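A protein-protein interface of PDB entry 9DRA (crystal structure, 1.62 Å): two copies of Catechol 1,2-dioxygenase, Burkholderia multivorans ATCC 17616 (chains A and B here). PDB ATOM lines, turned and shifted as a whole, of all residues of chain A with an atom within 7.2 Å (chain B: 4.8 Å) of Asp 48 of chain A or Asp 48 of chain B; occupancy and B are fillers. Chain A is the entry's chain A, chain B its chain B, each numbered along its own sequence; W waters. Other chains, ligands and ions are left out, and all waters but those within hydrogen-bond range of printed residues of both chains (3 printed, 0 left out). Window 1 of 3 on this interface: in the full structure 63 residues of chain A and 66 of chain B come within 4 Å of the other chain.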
ATOM      1  N   PHE A  14     -39.878  16.963  24.708  1.00  0.00           N
ATOM      2  CA  PHE A  14     -39.352  15.775  25.373  1.00  0.00           C
ATOM      3  C   PHE A  14     -40.229  15.349  26.545  1.00  0.00           C
ATOM      4  O   PHE A  14     -40.409  14.152  26.794  1.00  0.00           O
ATOM      5  CB  PHE A  14     -37.927  16.038  25.850  1.00  0.00           C
ATOM      6  CG  PHE A  14     -37.335  14.912  26.629  1.00  0.00           C
ATOM      7  CD1 PHE A  14     -36.834  13.784  25.986  1.00  0.00           C
ATOM      8  CD2 PHE A  14     -37.272  14.976  28.013  1.00  0.00           C
ATOM      9  CE1 PHE A  14     -36.262  12.733  26.727  1.00  0.00           C
ATOM     10  CE2 PHE A  14     -36.719  13.935  28.740  1.00  0.00           C
ATOM     11  CZ  PHE A  14     -36.219  12.811  28.093  1.00  0.00           C
ATOM     12  N   LEU A  23     -40.465   6.253  24.144  1.00  0.00           N
ATOM     13  CA  LEU A  23     -39.219   5.753  24.726  1.00  0.00           C
ATOM     14  C   LEU A  23     -39.437   4.441  25.467  1.00  0.00           C
ATOM     15  O   LEU A  23     -38.597   3.532  25.404  1.00  0.00           O
ATOM     16  CB  LEU A  23     -38.636   6.797  25.674  1.00  0.00           C
ATOM     17  CG  LEU A  23     -37.987   8.000  24.990  1.00  0.00           C
ATOM     18  CD1 LEU A  23     -37.841   9.157  25.932  1.00  0.00           C
ATOM     19  CD2 LEU A  23     -36.622   7.599  24.417  1.00  0.00           C
ATOM     20  N   VAL A  42     -30.464   0.835  27.417  1.00  0.00           N
ATOM     21  CA  VAL A  42     -30.988   1.382  26.168  1.00  0.00           C
ATOM     22  C   VAL A  42     -31.974   2.512  26.455  1.00  0.00           C
ATOM     23  O   VAL A  42     -31.935   3.565  25.812  1.00  0.00           O
ATOM     24  CB  VAL A  42     -31.627   0.273  25.304  1.00  0.00           C
ATOM     25  CG1 VAL A  42     -32.436   0.880  24.162  1.00  0.00           C
ATOM     26  CG2 VAL A  42     -30.567  -0.645  24.730  1.00  0.00           C
ATOM     27  N   HIS A  43     -32.845   2.348  27.449  1.00  0.00           N
ATOM     28  CA  HIS A  43     -33.778   3.430  27.719  1.00  0.00           C
ATOM     29  C   HIS A  43     -33.038   4.695  28.134  1.00  0.00           C
ATOM     30  O   HIS A  43     -33.413   5.803  27.730  1.00  0.00           O
ATOM     31  CB  HIS A  43     -34.782   3.025  28.780  1.00  0.00           C
ATOM     32  CG  HIS A  43     -35.839   4.052  29.019  1.00  0.00           C
ATOM     33  ND1 HIS A  43     -35.775   4.956  30.059  1.00  0.00           N
ATOM     34  CD2 HIS A  43     -36.985   4.327  28.352  1.00  0.00           C
ATOM     35  CE1 HIS A  43     -36.843   5.734  30.032  1.00  0.00           C
ATOM     36  NE2 HIS A  43     -37.598   5.372  29.006  1.00  0.00           N
ATOM     37  N   ARG A  44     -31.988   4.553  28.951  1.00  0.00           N
ATOM     38  CA  ARG A  44     -31.288   5.734  29.431  1.00  0.00           C
ATOM     39  C   ARG A  44     -30.583   6.447  28.291  1.00  0.00           C
ATOM     40  O   ARG A  44     -30.671   7.677  28.172  1.00  0.00           O
ATOM     41  CB  ARG A  44     -30.292   5.321  30.509  1.00  0.00           C
ATOM     42  CG  ARG A  44     -29.310   6.418  30.945  1.00  0.00           C
ATOM     43  CD  ARG A  44     -30.043   7.664  31.441  1.00  0.00           C
ATOM     44  NE  ARG A  44     -29.088   8.670  31.889  1.00  0.00           N
ATOM     45  CZ  ARG A  44     -28.626   8.766  33.127  1.00  0.00           C
ATOM     46  NH1 ARG A  44     -29.038   7.952  34.086  1.00  0.00           N
ATOM     47  NH2 ARG A  44     -27.721   9.696  33.406  1.00  0.00           N
ATOM     48  N   LEU A  45     -29.913   5.690  27.420  1.00  0.00           N
ATOM     49  CA  LEU A  45     -29.165   6.316  26.337  1.00  0.00           C
ATOM     50  C   LEU A  45     -30.110   6.955  25.323  1.00  0.00           C
ATOM     51  O   LEU A  45     -29.827   8.042  24.801  1.00  0.00           O
ATOM     52  CB  LEU A  45     -28.267   5.282  25.657  1.00  0.00           C
ATOM     53  CG  LEU A  45     -27.132   4.734  26.534  1.00  0.00           C
ATOM     54  CD1 LEU A  45     -26.304   3.727  25.762  1.00  0.00           C
ATOM     55  CD2 LEU A  45     -26.261   5.847  27.031  1.00  0.00           C
ATOM     56  N   LEU A  46     -31.220   6.277  25.022  1.00  0.00           N
ATOM     57  CA  LEU A  46     -32.202   6.830  24.096  1.00  0.00           C
ATOM     58  C   LEU A  46     -32.849   8.083  24.671  1.00  0.00           C
ATOM     59  O   LEU A  46     -32.997   9.098  23.974  1.00  0.00           O
ATOM     60  CB  LEU A  46     -33.250   5.761  23.783  1.00  0.00           C
ATOM     61  CG  LEU A  46     -34.189   6.024  22.618  1.00  0.00           C
ATOM     62  CD1 LEU A  46     -33.418   6.068  21.303  1.00  0.00           C
ATOM     63  CD2 LEU A  46     -35.259   4.941  22.567  1.00  0.00           C
ATOM     64  N   SER A  47     -33.225   8.040  25.950  1.00  0.00           N
ATOM     65  CA  SER A  47     -33.819   9.207  26.589  1.00  0.00           C
ATOM     66  C   SER A  47     -32.858  10.387  26.554  1.00  0.00           C
ATOM     67  O   SER A  47     -33.241  11.517  26.243  1.00  0.00           O
ATOM     68  CB  SER A  47     -34.204   8.863  28.027  1.00  0.00           C
ATOM     69  OG  SER A  47     -34.831   9.953  28.682  1.00  0.00           O
ATOM     70  N   ASP A  48     -31.599  10.141  26.878  1.00  0.00           N
ATOM     71  CA  ASP A  48     -30.641  11.229  26.873  1.00  0.00           C
ATOM     72  C   ASP A  48     -30.469  11.791  25.469  1.00  0.00           C
ATOM     73  O   ASP A  48     -30.371  13.011  25.290  1.00  0.00           O
ATOM     74  CB  ASP A  48     -29.306  10.732  27.416  1.00  0.00           C
ATOM     75  CG  ASP A  48     -29.305  10.525  28.924  1.00  0.00           C
ATOM     76  OD1 ASP A  48     -30.210  11.023  29.638  1.00  0.00           O
ATOM     77  OD2 ASP A  48     -28.350   9.860  29.387  1.00  0.00           O
ATOM     78  N   LEU A  49     -30.442  10.918  24.454  1.00  0.00           N
ATOM     79  CA  LEU A  49     -30.302  11.389  23.084  1.00  0.00           C
ATOM     80  C   LEU A  49     -31.499  12.241  22.698  1.00  0.00           C
ATOM     81  O   LEU A  49     -31.351  13.339  22.140  1.00  0.00           O
ATOM     82  CB  LEU A  49     -30.166  10.202  22.129  1.00  0.00           C
ATOM     83  CG  LEU A  49     -30.158  10.558  20.647  1.00  0.00           C
ATOM     84  CD1 LEU A  49     -28.974  11.428  20.280  1.00  0.00           C
ATOM     85  CD2 LEU A  49     -30.135   9.278  19.859  1.00  0.00           C
ATOM     86  N   PHE A  50     -32.703  11.764  23.026  1.00  0.00           N
ATOM     87  CA  PHE A  50     -33.898  12.529  22.680  1.00  0.00           C
ATOM     88  C   PHE A  50     -33.906  13.888  23.383  1.00  0.00           C
ATOM     89  O   PHE A  50     -34.306  14.894  22.789  1.00  0.00           O
ATOM     90  CB  PHE A  50     -35.180  11.759  23.032  1.00  0.00           C
ATOM     91  CG  PHE A  50     -35.556  10.631  22.056  1.00  0.00           C
ATOM     92  CD1 PHE A  50     -34.628  10.044  21.222  1.00  0.00           C
ATOM     93  CD2 PHE A  50     -36.868  10.165  22.024  1.00  0.00           C
ATOM     94  CE1 PHE A  50     -34.982   9.004  20.379  1.00  0.00           C
ATOM     95  CE2 PHE A  50     -37.236   9.128  21.178  1.00  0.00           C
ATOM     96  CZ  PHE A  50     -36.301   8.549  20.355  1.00  0.00           C
ATOM     97  N   LYS A  51     -33.467  13.943  24.653  1.00  0.00           N
ATOM     98  CA  LYS A  51     -33.459  15.212  25.367  1.00  0.00           C
ATOM     99  C   LYS A  51     -32.427  16.168  24.779  1.00  0.00           C
ATOM    100  O   LYS A  51     -32.672  17.377  24.697  1.00  0.00           O
ATOM    101  CB  LYS A  51     -33.199  14.971  26.853  1.00  0.00           C
ATOM    102  CG  LYS A  51     -33.312  16.214  27.717  1.00  0.00           C
ATOM    103  CD  LYS A  51     -33.332  15.857  29.185  1.00  0.00           C
ATOM    104  CE  LYS A  51     -33.832  17.024  30.012  1.00  0.00           C
ATOM    105  NZ  LYS A  51     -33.302  18.323  29.514  1.00  0.00           N
ATOM    106  N   ALA A  52     -31.259  15.647  24.382  1.00  0.00           N
ATOM    107  CA  ALA A  52     -30.243  16.495  23.773  1.00  0.00           C
ATOM    108  C   ALA A  52     -30.716  17.062  22.444  1.00  0.00           C
ATOM    109  O   ALA A  52     -30.458  18.229  22.140  1.00  0.00           O
ATOM    110  CB  ALA A  52     -28.942  15.704  23.582  1.00  0.00           C
ATOM    111  N   ILE A  53     -31.398  16.245  21.632  1.00  0.00           N
ATOM    112  CA  ILE A  53     -31.975  16.726  20.381  1.00  0.00           C
ATOM    113  C   ILE A  53     -32.965  17.857  20.655  1.00  0.00           C
ATOM    114  O   ILE A  53     -32.934  18.908  20.008  1.00  0.00           O
ATOM    115  CB  ILE A  53     -32.632  15.548  19.635  1.00  0.00           C
ATOM    116  CG1 ILE A  53     -31.547  14.606  19.088  1.00  0.00           C
ATOM    117  CG2 ILE A  53     -33.565  16.033  18.504  1.00  0.00           C
ATOM    118  CD1 ILE A  53     -32.080  13.305  18.477  1.00  0.00           C
ATOM    119  N   ASP A  54     -33.825  17.677  21.653  1.00  0.00           N
ATOM    120  CA  ASP A  54     -34.783  18.723  22.017  1.00  0.00           C
ATOM    121  C   ASP A  54     -34.063  19.977  22.532  1.00  0.00           C
ATOM    122  O   ASP A  54     -34.343  21.096  22.089  1.00  0.00           O
ATOM    123  CB  ASP A  54     -35.749  18.164  23.066  1.00  0.00           C
ATOM    124  CG  ASP A  54     -37.103  18.829  23.063  1.00  0.00           C
ATOM    125  OD1 ASP A  54     -37.671  19.060  21.969  1.00  0.00           O
ATOM    126  OD2 ASP A  54     -37.614  19.066  24.176  1.00  0.00           O
ATOM    127  N   ASP A  55     -33.101  19.804  23.447  1.00  0.00           N
ATOM    128  CA  ASP A  55     -32.473  20.953  24.098  1.00  0.00           C
ATOM    129  C   ASP A  55     -31.648  21.804  23.135  1.00  0.00           C
ATOM    130  O   ASP A  55     -31.612  23.039  23.269  1.00  0.00           O
ATOM    131  CB  ASP A  55     -31.554  20.490  25.225  1.00  0.00           C
ATOM    132  CG  ASP A  55     -32.288  20.091  26.474  1.00  0.00           C
ATOM    133  OD1 ASP A  55     -33.506  20.344  26.572  1.00  0.00           O
ATOM    134  OD2 ASP A  55     -31.617  19.543  27.377  1.00  0.00           O
ATOM    135  N   ARG B  44     -22.035  17.814  24.376  1.00  0.00           N
ATOM    136  CA  ARG B  44     -23.254  17.395  25.057  1.00  0.00           C
ATOM    137  C   ARG B  44     -23.433  15.878  25.000  1.00  0.00           C
ATOM    138  O   ARG B  44     -23.777  15.249  26.006  1.00  0.00           O
ATOM    139  CB  ARG B  44     -24.458  18.102  24.425  1.00  0.00           C
ATOM    140  CG  ARG B  44     -25.800  17.600  24.910  1.00  0.00           C
ATOM    141  CD  ARG B  44     -25.986  17.823  26.395  1.00  0.00           C
ATOM    142  NE  ARG B  44     -27.316  17.370  26.791  1.00  0.00           N
ATOM    143  CZ  ARG B  44     -28.395  18.135  26.877  1.00  0.00           C
ATOM    144  NH1 ARG B  44     -28.350  19.438  26.637  1.00  0.00           N
ATOM    145  NH2 ARG B  44     -29.559  17.574  27.192  1.00  0.00           N
ATOM    146  N   LEU B  45     -23.301  15.283  23.812  1.00  0.00           N
ATOM    147  CA  LEU B  45     -23.482  13.836  23.696  1.00  0.00           C
ATOM    148  C   LEU B  45     -22.465  13.059  24.529  1.00  0.00           C
ATOM    149  O   LEU B  45     -22.812  12.054  25.172  1.00  0.00           O
ATOM    150  CB  LEU B  45     -23.410  13.432  22.227  1.00  0.00           C
ATOM    151  CG  LEU B  45     -24.566  13.948  21.361  1.00  0.00           C
ATOM    152  CD1 LEU B  45     -24.331  13.468  19.944  1.00  0.00           C
ATOM    153  CD2 LEU B  45     -25.907  13.501  21.864  1.00  0.00           C
ATOM    154  N   LEU B  46     -21.201  13.500  24.535  1.00  0.00           N
ATOM    155  CA  LEU B  46     -20.177  12.813  25.321  1.00  0.00           C
ATOM    156  C   LEU B  46     -20.427  12.982  26.809  1.00  0.00           C
ATOM    157  O   LEU B  46     -20.301  12.028  27.587  1.00  0.00           O
ATOM    158  CB  LEU B  46     -18.797  13.355  24.980  1.00  0.00           C
ATOM    159  CG  LEU B  46     -18.202  13.036  23.619  1.00  0.00           C
ATOM    160  CD1 LEU B  46     -16.848  13.702  23.558  1.00  0.00           C
ATOM    161  CD2 LEU B  46     -18.089  11.537  23.442  1.00  0.00           C
ATOM    162  N   SER B  47     -20.798  14.184  27.216  1.00  0.00           N
ATOM    163  CA  SER B  47     -21.097  14.413  28.622  1.00  0.00           C
ATOM    164  C   SER B  47     -22.257  13.539  29.080  1.00  0.00           C
ATOM    165  O   SER B  47     -22.195  12.925  30.144  1.00  0.00           O
ATOM    166  CB  SER B  47     -21.401  15.888  28.850  1.00  0.00           C
ATOM    167  OG  SER B  47     -21.568  16.151  30.230  1.00  0.00           O
ATOM    168  N   ASP B  48     -23.322  13.450  28.276  1.00  0.00           N
ATOM    169  CA  ASP B  48     -24.432  12.612  28.686  1.00  0.00           C
ATOM    170  C   ASP B  48     -24.008  11.153  28.768  1.00  0.00           C
ATOM    171  O   ASP B  48     -24.468  10.421  29.648  1.00  0.00           O
ATOM    172  CB  ASP B  48     -25.582  12.752  27.709  1.00  0.00           C
ATOM    173  CG  ASP B  48     -26.305  14.091  27.828  1.00  0.00           C
ATOM    174  OD1 ASP B  48     -26.156  14.795  28.855  1.00  0.00           O
ATOM    175  OD2 ASP B  48     -27.033  14.419  26.865  1.00  0.00           O
ATOM    176  N   LEU B  49     -23.193  10.698  27.808  1.00  0.00           N
ATOM    177  CA  LEU B  49     -22.701   9.322  27.828  1.00  0.00           C
ATOM    178  C   LEU B  49     -21.862   9.060  29.073  1.00  0.00           C
ATOM    179  O   LEU B  49     -22.053   8.054  29.770  1.00  0.00           O
ATOM    180  CB  LEU B  49     -21.886   9.040  26.560  1.00  0.00           C
ATOM    181  CG  LEU B  49     -21.228   7.668  26.538  1.00  0.00           C
ATOM    182  CD1 LEU B  49     -22.269   6.559  26.609  1.00  0.00           C
ATOM    183  CD2 LEU B  49     -20.352   7.559  25.297  1.00  0.00           C
ATOM    184  N   PHE B  50     -20.944   9.962  29.386  1.00  0.00           N
ATOM    185  CA  PHE B  50     -20.121   9.759  30.578  1.00  0.00           C
ATOM    186  C   PHE B  50     -20.989   9.746  31.844  1.00  0.00           C
ATOM    187  O   PHE B  50     -20.753   8.962  32.775  1.00  0.00           O
ATOM    188  CB  PHE B  50     -19.058  10.858  30.710  1.00  0.00           C
ATOM    189  CG  PHE B  50     -17.876  10.740  29.778  1.00  0.00           C
ATOM    190  CD1 PHE B  50     -17.942  10.030  28.598  1.00  0.00           C
ATOM    191  CD2 PHE B  50     -16.690  11.396  30.099  1.00  0.00           C
ATOM    192  CE1 PHE B  50     -16.844   9.968  27.742  1.00  0.00           C
ATOM    193  CE2 PHE B  50     -15.595  11.327  29.249  1.00  0.00           C
ATOM    194  CZ  PHE B  50     -15.688  10.611  28.074  1.00  0.00           C
ATOM    195  N   LYS B  51     -21.976  10.634  31.911  1.00  0.00           N
ATOM    196  CA  LYS B  51     -22.842  10.667  33.087  1.00  0.00           C
ATOM    197  C   LYS B  51     -23.658   9.387  33.186  1.00  0.00           C
ATOM    198  O   LYS B  51     -23.851   8.855  34.276  1.00  0.00           O
ATOM    199  CB  LYS B  51     -23.744  11.898  33.041  1.00  0.00           C
ATOM    200  CG  LYS B  51     -24.793  11.953  34.152  1.00  0.00           C
ATOM    201  CD  LYS B  51     -25.482  13.295  34.194  1.00  0.00           C
ATOM    202  CE  LYS B  51     -26.470  13.383  35.356  1.00  0.00           C
ATOM    203  NZ  LYS B  51     -25.808  13.147  36.654  1.00  0.00           N
ATOM    204  N   ALA B  52     -24.135   8.864  32.049  1.00  0.00           N
ATOM    205  CA  ALA B  52     -24.897   7.624  32.107  1.00  0.00           C
ATOM    206  C   ALA B  52     -24.035   6.450  32.547  1.00  0.00           C
ATOM    207  O   ALA B  52     -24.490   5.580  33.294  1.00  0.00           O
ATOM    208  CB  ALA B  52     -25.543   7.342  30.740  1.00  0.00           C
HETATM  209  O   HOH W   1     -26.622  11.049  31.000  1.00  0.00           O
HETATM  210  O   HOH W   2     -26.307   8.957  27.418  1.00  0.00           O
HETATM  211  O   HOH W   3     -29.597  14.584  27.467  1.00  0.00           O
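The side-chain amino group (NZ) of Lys 51 of chain A is in salt-bridge range of the side-chain carboxylate (OD2) of Asp 55 of chain A (3.0 Å). The guanidinium group (NE) of Arg 44 of chain A lies within salt-bridge range of the side-chain carboxylate (OD2) of Asp 48 of chain A (2.9 Å). NE of Arg 44 of chain B lies within salt-bridge range of OD2 of Asp 48 of chain B (3.0 Å).
Among the printed residues, 6 pairs touch across the chains.
Printed residues of chain B within 4 Å of Asp 48 of chain A: Asp 48 (3.9 Å). Of the printed residues of chain A, Asp 48 of chain B touches Asp 48. Of the printed residues of chain B, Lys 51 of chain A touches Arg 44 (3.99 Å). Printed residues of chain B within 4 Å of Asp 55 of chain A: Arg 44. Of the printed residues of chain A, Lys 51 of chain B touches Arg 44 (3.8 Å). Leu 46 of chain B touches none of the printed residues of chain A. Asp 54 of chain A touches none of the printed residues of chain B. The nearest printed residue of chain B that does not touch Asp 48 of chain A is Ala 52 of chain B (4.01 Å). The nearest printed residue of chain A that does not touch Asp 48 of chain B is Ala 52 of chain A (4.01 Å).
Lys 51 of chain B touches Arg 44 of chain A. NH2 of Arg 44 of chain A touches CA of Ala 52 of chain B, 3.7 Å away. OD2 of Asp 48 of chain A touches O of Asp 48 of chain B (3.9 Å). Lys 51 of chain A touches Arg 44 of chain B (O to NH2, 3.99 Å). NH2 of Arg 44 of chain B touches CA of Ala 52 of chain A, 3.6 Å away.
Arg 44 of chain A touches Lys 51 of chain B, and with the chains exchanged Lys 51 of chain A touches Arg 44 of chain B. Arg 44 of chain A touches Ala 52 of chain B, and with the chains exchanged Ala 52 of chain A touches Arg 44 of chain B. Asp 48 of chain B touches its own counterpart, Asp 48 of chain A. Of the 6 pairs that touch across the chains among the printed residues, 5 have their exchanged pair printed and touching as well.
Water W1 lies within hydrogen-bond range of O of Asp 48 of chain B (2.6 Å), OD2 of Asp 48 of chain A (2.6 Å), NH2 of Arg 44 of chain A (3.0 Å) and N of Ala 52 of chain B (3.5 Å). Water W3 lies within hydrogen-bond range of the side-chain carboxylate of Asp 48 of chain B (2.6 Å), the backbone carbonyl oxygen of Asp 48 of chain A (2.8 Å) and the guanidinium group of Arg 44 of chain B (3.0 Å). Water W2 bridges the side-chain carboxylate (OD2) of Asp 48 of chain A (3.0 Å) and the backbone carbonyl oxygen (O) of Asp 48 of chain B (3.2 Å).
The side-chain carboxylate (OD2) of Asp 55 of chain A is in salt-bridge range of the guanidinium group (NH2) of Arg 44 of chain B (2.9 Å).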
